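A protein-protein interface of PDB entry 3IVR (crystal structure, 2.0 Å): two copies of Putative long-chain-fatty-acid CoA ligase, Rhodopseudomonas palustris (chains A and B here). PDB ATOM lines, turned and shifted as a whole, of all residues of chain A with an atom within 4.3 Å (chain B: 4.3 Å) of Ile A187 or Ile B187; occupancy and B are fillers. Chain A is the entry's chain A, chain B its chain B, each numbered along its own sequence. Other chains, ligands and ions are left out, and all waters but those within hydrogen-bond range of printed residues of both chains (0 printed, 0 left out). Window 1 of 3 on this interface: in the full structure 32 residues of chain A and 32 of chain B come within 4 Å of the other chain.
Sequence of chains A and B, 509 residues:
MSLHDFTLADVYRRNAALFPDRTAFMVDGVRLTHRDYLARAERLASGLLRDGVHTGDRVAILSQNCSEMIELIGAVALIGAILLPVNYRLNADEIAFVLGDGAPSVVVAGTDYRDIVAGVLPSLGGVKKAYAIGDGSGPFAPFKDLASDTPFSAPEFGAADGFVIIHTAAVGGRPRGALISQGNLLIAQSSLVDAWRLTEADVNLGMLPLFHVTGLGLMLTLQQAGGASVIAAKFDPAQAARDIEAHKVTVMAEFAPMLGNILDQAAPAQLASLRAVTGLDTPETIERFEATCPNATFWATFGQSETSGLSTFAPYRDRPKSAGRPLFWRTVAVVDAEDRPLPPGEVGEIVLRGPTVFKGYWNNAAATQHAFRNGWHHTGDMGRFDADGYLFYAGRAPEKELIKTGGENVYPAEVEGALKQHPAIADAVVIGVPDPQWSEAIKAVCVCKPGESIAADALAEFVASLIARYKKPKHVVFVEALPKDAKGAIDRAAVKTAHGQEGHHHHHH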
ATOM      1  N   GLY A 183      26.393  23.400 -11.564  1.00  0.00           N
ATOM      2  CA  GLY A 183      26.315  21.945 -11.492  1.00  0.00           C
ATOM      3  C   GLY A 183      25.201  21.445 -10.597  1.00  0.00           C
ATOM      4  O   GLY A 183      24.525  20.473 -10.945  1.00  0.00           O
ATOM      5  N   ASN A 184      25.017  22.095  -9.448  1.00  0.00           N
ATOM      6  CA  ASN A 184      23.857  21.835  -8.568  1.00  0.00           C
ATOM      7  C   ASN A 184      22.592  21.779  -9.413  1.00  0.00           C
ATOM      8  O   ASN A 184      21.891  20.771  -9.415  1.00  0.00           O
ATOM      9  CB  ASN A 184      23.651  22.976  -7.574  1.00  0.00           C
ATOM     10  CG  ASN A 184      24.532  22.914  -6.331  1.00  0.00           C
ATOM     11  OD1 ASN A 184      24.900  23.968  -5.812  1.00  0.00           O
ATOM     12  ND2 ASN A 184      24.804  21.709  -5.794  1.00  0.00           N
ATOM     13  N   LEU A 185      22.311  22.875 -10.137  1.00  0.00           N
ATOM     14  CA  LEU A 185      21.104  22.990 -10.956  1.00  0.00           C
ATOM     15  C   LEU A 185      21.065  21.994 -12.094  1.00  0.00           C
ATOM     16  O   LEU A 185      20.055  21.344 -12.296  1.00  0.00           O
ATOM     17  CB  LEU A 185      20.913  24.410 -11.495  1.00  0.00           C
ATOM     18  CG  LEU A 185      20.685  25.501 -10.439  1.00  0.00           C
ATOM     19  CD1 LEU A 185      20.632  26.870 -11.105  1.00  0.00           C
ATOM     20  CD2 LEU A 185      19.418  25.245  -9.602  1.00  0.00           C
ATOM     21  N   LEU A 186      22.158  21.853 -12.833  1.00  0.00           N
ATOM     22  CA  LEU A 186      22.133  20.943 -13.968  1.00  0.00           C
ATOM     23  C   LEU A 186      21.814  19.521 -13.522  1.00  0.00           C
ATOM     24  O   LEU A 186      20.979  18.854 -14.118  1.00  0.00           O
ATOM     25  CB  LEU A 186      23.459  20.973 -14.733  1.00  0.00           C
ATOM     26  CG  LEU A 186      23.755  22.242 -15.528  1.00  0.00           C
ATOM     27  CD1 LEU A 186      25.161  22.206 -16.089  1.00  0.00           C
ATOM     28  CD2 LEU A 186      22.742  22.401 -16.641  1.00  0.00           C
ATOM     29  N   ILE A 187      22.482  19.061 -12.468  1.00  0.00           N
ATOM     30  CA  ILE A 187      22.286  17.692 -12.028  1.00  0.00           C
ATOM     31  C   ILE A 187      20.905  17.501 -11.392  1.00  0.00           C
ATOM     32  O   ILE A 187      20.225  16.520 -11.695  1.00  0.00           O
ATOM     33  CB  ILE A 187      23.509  17.115 -11.207  1.00  0.00           C
ATOM     34  CG1 ILE A 187      23.492  15.589 -11.244  1.00  0.00           C
ATOM     35  CG2 ILE A 187      23.575  17.623  -9.785  1.00  0.00           C
ATOM     36  CD1 ILE A 187      24.859  14.957 -10.994  1.00  0.00           C
ATOM     37  N   ALA A 188      20.474  18.461 -10.568  1.00  0.00           N
ATOM     38  CA  ALA A 188      19.118  18.420  -9.990  1.00  0.00           C
ATOM     39  C   ALA A 188      18.037  18.315 -11.075  1.00  0.00           C
ATOM     40  O   ALA A 188      17.165  17.440 -11.019  1.00  0.00           O
ATOM     41  CB  ALA A 188      18.861  19.619  -9.069  1.00  0.00           C
ATOM     42  N   GLN A 189      18.169  19.147 -12.101  1.00  0.00           N
ATOM     43  CA  GLN A 189      17.182  19.249 -13.159  1.00  0.00           C
ATOM     44  C   GLN A 189      17.231  18.133 -14.188  1.00  0.00           C
ATOM     45  O   GLN A 189      16.246  17.912 -14.874  1.00  0.00           O
ATOM     46  CB  GLN A 189      17.255  20.616 -13.827  1.00  0.00           C
ATOM     47  CG  GLN A 189      16.956  21.730 -12.852  1.00  0.00           C
ATOM     48  CD  GLN A 189      17.604  23.055 -13.205  1.00  0.00           C
ATOM     49  OE1 GLN A 189      17.562  23.961 -12.400  1.00  0.00           O
ATOM     50  NE2 GLN A 189      18.218  23.170 -14.402  1.00  0.00           N
ATOM     51  N   SER A 190      18.347  17.407 -14.272  1.00  0.00           N
ATOM     52  CA  SER A 190      18.452  16.245 -15.169  1.00  0.00           C
ATOM     53  C   SER A 190      17.440  15.140 -14.794  1.00  0.00           C
ATOM     54  O   SER A 190      17.031  14.306 -15.627  1.00  0.00           O
ATOM     55  CB  SER A 190      19.893  15.687 -15.177  1.00  0.00           C
ATOM     56  OG  SER A 190      20.237  15.111 -13.918  1.00  0.00           O
ATOM     57  N   SER A 191      17.040  15.155 -13.534  1.00  0.00           N
ATOM     58  CA  SER A 191      16.070  14.213 -12.995  1.00  0.00           C
ATOM     59  C   SER A 191      14.645  14.563 -13.398  1.00  0.00           C
ATOM     60  O   SER A 191      13.803  13.672 -13.537  1.00  0.00           O
ATOM     61  CB  SER A 191      16.179  14.179 -11.469  1.00  0.00           C
ATOM     62  OG  SER A 191      17.461  13.698 -11.089  1.00  0.00           O
ATOM     63  N   TRP A 329      20.281  10.928  -7.394  1.00  0.00           N
ATOM     64  CA  TRP A 329      21.226  11.975  -6.921  1.00  0.00           C
ATOM     65  C   TRP A 329      20.985  12.498  -5.518  1.00  0.00           C
ATOM     66  O   TRP A 329      21.795  13.268  -5.011  1.00  0.00           O
ATOM     67  CB  TRP A 329      21.414  13.158  -7.909  1.00  0.00           C
ATOM     68  CG  TRP A 329      21.717  12.775  -9.343  1.00  0.00           C
ATOM     69  CD1 TRP A 329      20.914  12.974 -10.419  1.00  0.00           C
ATOM     70  CD2 TRP A 329      22.910  12.137  -9.844  1.00  0.00           C
ATOM     71  NE1 TRP A 329      21.534  12.518 -11.574  1.00  0.00           N
ATOM     72  CE2 TRP A 329      22.753  11.994 -11.243  1.00  0.00           C
ATOM     73  CE3 TRP A 329      24.104  11.690  -9.246  1.00  0.00           C
ATOM     74  CZ2 TRP A 329      23.736  11.416 -12.057  1.00  0.00           C
ATOM     75  CZ3 TRP A 329      25.083  11.100 -10.062  1.00  0.00           C
ATOM     76  CH2 TRP A 329      24.894  10.984 -11.442  1.00  0.00           C
ATOM     77  N   PRO A 355      24.991  15.748  -4.703  1.00  0.00           N
ATOM     78  CA  PRO A 355      25.466  16.892  -5.486  1.00  0.00           C
ATOM     79  C   PRO A 355      24.403  17.971  -5.764  1.00  0.00           C
ATOM     80  O   PRO A 355      24.711  18.951  -6.453  1.00  0.00           O
ATOM     81  CB  PRO A 355      25.925  16.242  -6.801  1.00  0.00           C
ATOM     82  CG  PRO A 355      25.092  15.007  -6.924  1.00  0.00           C
ATOM     83  CD  PRO A 355      24.809  14.543  -5.528  1.00  0.00           C
ATOM     84  N   THR A 356      23.185  17.799  -5.236  1.00  0.00           N
ATOM     85  CA  THR A 356      22.126  18.815  -5.358  1.00  0.00           C
ATOM     86  C   THR A 356      22.079  19.750  -4.149  1.00  0.00           C
ATOM     87  O   THR A 356      21.419  20.794  -4.193  1.00  0.00           O
ATOM     88  CB  THR A 356      20.704  18.214  -5.601  1.00  0.00           C
ATOM     89  OG1 THR A 356      20.213  17.575  -4.411  1.00  0.00           O
ATOM     90  CG2 THR A 356      20.700  17.226  -6.779  1.00  0.00           C
ATOM     91  N   GLY B 183      31.688   8.379 -10.357  1.00  0.00           N
ATOM     92  CA  GLY B 183      30.987   9.543 -10.873  1.00  0.00           C
ATOM     93  C   GLY B 183      30.938   9.585 -12.389  1.00  0.00           C
ATOM     94  O   GLY B 183      29.888   9.864 -12.949  1.00  0.00           O
ATOM     95  N   ASN B 184      32.065   9.280 -13.041  1.00  0.00           N
ATOM     96  CA  ASN B 184      32.122   9.130 -14.489  1.00  0.00           C
ATOM     97  C   ASN B 184      31.000   8.216 -14.992  1.00  0.00           C
ATOM     98  O   ASN B 184      30.293   8.572 -15.921  1.00  0.00           O
ATOM     99  CB  ASN B 184      33.413   8.436 -14.929  1.00  0.00           C
ATOM    100  CG  ASN B 184      34.629   9.339 -15.004  1.00  0.00           C
ATOM    101  OD1 ASN B 184      35.737   8.855 -14.766  1.00  0.00           O
ATOM    102  ND2 ASN B 184      34.463  10.607 -15.402  1.00  0.00           N
ATOM    103  N   LEU B 185      30.880   7.028 -14.391  1.00  0.00           N
ATOM    104  CA  LEU B 185      29.906   6.026 -14.806  1.00  0.00           C
ATOM    105  C   LEU B 185      28.484   6.468 -14.504  1.00  0.00           C
ATOM    106  O   LEU B 185      27.653   6.438 -15.389  1.00  0.00           O
ATOM    107  CB  LEU B 185      30.187   4.632 -14.192  1.00  0.00           C
ATOM    108  CG  LEU B 185      31.493   3.954 -14.617  1.00  0.00           C
ATOM    109  CD1 LEU B 185      31.737   2.733 -13.764  1.00  0.00           C
ATOM    110  CD2 LEU B 185      31.473   3.575 -16.083  1.00  0.00           C
ATOM    111  N   LEU B 186      28.205   6.886 -13.273  1.00  0.00           N
ATOM    112  CA  LEU B 186      26.852   7.319 -12.922  1.00  0.00           C
ATOM    113  C   LEU B 186      26.308   8.425 -13.844  1.00  0.00           C
ATOM    114  O   LEU B 186      25.156   8.359 -14.302  1.00  0.00           O
ATOM    115  CB  LEU B 186      26.772   7.770 -11.457  1.00  0.00           C
ATOM    116  CG  LEU B 186      27.068   6.725 -10.373  1.00  0.00           C
ATOM    117  CD1 LEU B 186      27.359   7.416  -9.043  1.00  0.00           C
ATOM    118  CD2 LEU B 186      25.960   5.730 -10.234  1.00  0.00           C
ATOM    119  N   ILE B 187      27.145   9.422 -14.129  1.00  0.00           N
ATOM    120  CA  ILE B 187      26.694  10.562 -14.906  1.00  0.00           C
ATOM    121  C   ILE B 187      26.500  10.145 -16.355  1.00  0.00           C
ATOM    122  O   ILE B 187      25.487  10.491 -16.956  1.00  0.00           O
ATOM    123  CB  ILE B 187      27.556  11.863 -14.688  1.00  0.00           C
ATOM    124  CG1 ILE B 187      26.729  13.096 -15.063  1.00  0.00           C
ATOM    125  CG2 ILE B 187      28.895  11.831 -15.453  1.00  0.00           C
ATOM    126  CD1 ILE B 187      27.069  14.317 -14.260  1.00  0.00           C
ATOM    127  N   ALA B 188      27.412   9.322 -16.870  1.00  0.00           N
ATOM    128  CA  ALA B 188      27.371   8.899 -18.263  1.00  0.00           C
ATOM    129  C   ALA B 188      26.142   8.054 -18.524  1.00  0.00           C
ATOM    130  O   ALA B 188      25.484   8.195 -19.561  1.00  0.00           O
ATOM    131  CB  ALA B 188      28.614   8.122 -18.628  1.00  0.00           C
ATOM    132  N   GLN B 189      25.837   7.193 -17.560  1.00  0.00           N
ATOM    133  CA  GLN B 189      24.787   6.204 -17.700  1.00  0.00           C
ATOM    134  C   GLN B 189      23.409   6.783 -17.419  1.00  0.00           C
ATOM    135  O   GLN B 189      22.398   6.226 -17.852  1.00  0.00           O
ATOM    136  CB  GLN B 189      25.074   5.009 -16.798  1.00  0.00           C
ATOM    137  CG  GLN B 189      26.312   4.234 -17.238  1.00  0.00           C
ATOM    138  CD  GLN B 189      26.963   3.382 -16.137  1.00  0.00           C
ATOM    139  OE1 GLN B 189      27.980   2.760 -16.378  1.00  0.00           O
ATOM    140  NE2 GLN B 189      26.396   3.376 -14.932  1.00  0.00           N
ATOM    141  N   SER B 190      23.369   7.913 -16.720  1.00  0.00           N
ATOM    142  CA  SER B 190      22.103   8.614 -16.473  1.00  0.00           C
ATOM    143  C   SER B 190      21.434   9.039 -17.802  1.00  0.00           C
ATOM    144  O   SER B 190      20.211   9.031 -17.927  1.00  0.00           O
ATOM    145  CB  SER B 190      22.308   9.801 -15.527  1.00  0.00           C
ATOM    146  OG  SER B 190      23.039  10.844 -16.161  1.00  0.00           O
ATOM    147  N   SER B 191      22.249   9.368 -18.790  1.00  0.00           N
ATOM    148  CA  SER B 191      21.785   9.652 -20.155  1.00  0.00           C
ATOM    149  C   SER B 191      21.114   8.471 -20.852  1.00  0.00           C
ATOM    150  O   SER B 191      20.195   8.666 -21.640  1.00  0.00           O
ATOM    151  CB  SER B 191      22.952  10.163 -20.990  1.00  0.00           C
ATOM    152  OG  SER B 191      23.530  11.289 -20.353  1.00  0.00           O
ATOM    153  N   TRP B 329      25.723  16.051 -21.186  1.00  0.00           N
ATOM    154  CA  TRP B 329      26.959  15.948 -20.395  1.00  0.00           C
ATOM    155  C   TRP B 329      28.233  15.824 -21.246  1.00  0.00           C
ATOM    156  O   TRP B 329      29.343  15.917 -20.701  1.00  0.00           O
ATOM    157  CB  TRP B 329      26.938  14.844 -19.309  1.00  0.00           C
ATOM    158  CG  TRP B 329      25.775  14.889 -18.324  1.00  0.00           C
ATOM    159  CD1 TRP B 329      24.776  13.989 -18.227  1.00  0.00           C
ATOM    160  CD2 TRP B 329      25.522  15.875 -17.323  1.00  0.00           C
ATOM    161  NE1 TRP B 329      23.900  14.332 -17.218  1.00  0.00           N
ATOM    162  CE2 TRP B 329      24.337  15.492 -16.645  1.00  0.00           C
ATOM    163  CE3 TRP B 329      26.167  17.065 -16.942  1.00  0.00           C
ATOM    164  CZ2 TRP B 329      23.791  16.237 -15.610  1.00  0.00           C
ATOM    165  CZ3 TRP B 329      25.634  17.797 -15.900  1.00  0.00           C
ATOM    166  CH2 TRP B 329      24.464  17.371 -15.234  1.00  0.00           C
ATOM    167  N   PRO B 355      32.204  15.689 -17.840  1.00  0.00           N
ATOM    168  CA  PRO B 355      32.342  14.797 -16.678  1.00  0.00           C
ATOM    169  C   PRO B 355      32.281  13.297 -16.982  1.00  0.00           C
ATOM    170  O   PRO B 355      32.406  12.505 -16.058  1.00  0.00           O
ATOM    171  CB  PRO B 355      31.156  15.210 -15.772  1.00  0.00           C
ATOM    172  CG  PRO B 355      30.127  15.789 -16.715  1.00  0.00           C
ATOM    173  CD  PRO B 355      30.906  16.407 -17.851  1.00  0.00           C
ATOM    174  N   THR B 356      32.095  12.922 -18.250  1.00  0.00           N
ATOM    175  CA  THR B 356      32.179  11.517 -18.674  1.00  0.00           C
ATOM    176  C   THR B 356      33.607  11.123 -19.099  1.00  0.00           C
ATOM    177  O   THR B 356      33.903   9.950 -19.225  1.00  0.00           O
ATOM    178  CB  THR B 356      31.124  11.156 -19.776  1.00  0.00           C
ATOM    179  OG1 THR B 356      31.456  11.782 -21.025  1.00  0.00           O
ATOM    180  CG2 THR B 356      29.683  11.585 -19.336  1.00  0.00           C
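Printed residues of chain B within 4 Å of Ile A187: Ile B187 (3.995 Å) and Trp B329 (3.8 Å). Of the printed residues of chain A, Ile B187 touches Ile A187 (3.995 Å) and Trp A329 (3.8 Å). Of the printed residues of chain B, Trp A329 touches Leu B186 (3.7 Å) and Ile B187 (3.8 Å). Of the printed residues of chain A, Leu B186 touches Trp A329. Of the printed residues of chain B, Leu A186 touches Trp B329 (3.8 Å). Of the printed residues of chain A, Trp B329 touches Leu A186, Ile A187 and Ser A190. Printed residues of chain B within 4 Å of Ser A190: Trp B329. The nearest printed residue of chain A that does not touch Ile B187 is Ser A190 (6.9 Å).
O of Ile A187 is in hydrogen-bond range of OG of Ser A190 (2.6 Å). O of Ile B187 is in hydrogen-bond range of OG of Ser B190 (2.6 Å).
Among the printed residues, merely in contact across the chains: Trp A329 with Leu B186 (3.7 Å), Leu A186 with Trp B329 (3.8 Å), Ile A187 with Trp B329 (3.8 Å), Trp A329 with Ile B187 (3.8 Å), Ser A190 with Trp B329 (3.96 Å) and Ile A187 with Ile B187 (3.995 Å).
Printed residues of chain B that touch a printed residue of chain A: Leu B186, Ile B187 and Trp B329. Printed residues of chain A that touch a printed residue of chain B: Leu A186, Ile A187, Ser A190 and Trp A329. Hydrophobic or aromatic side chains of chain A within 4 Å of the printed part of chain B: Leu A186, Ile A187 and Trp A329. Along chain A the printed residues that touch a printed residue of chain B span positions 186 to 329. Among the printed residues, 6 pairs touch across the chains.
Leu A186 touches Trp B329, and with the chains exchanged Trp A329 touches Leu B186. Ile B187 touches its own counterpart, Ile A187. Ile A187 touches Trp B329, and with the chains exchanged Trp A329 touches Ile B187. Ser A190 touches Trp B329, but with the chains exchanged Trp A329 does not touch Ser B190 (4.1 Å). 12 positions are printed for both chains.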
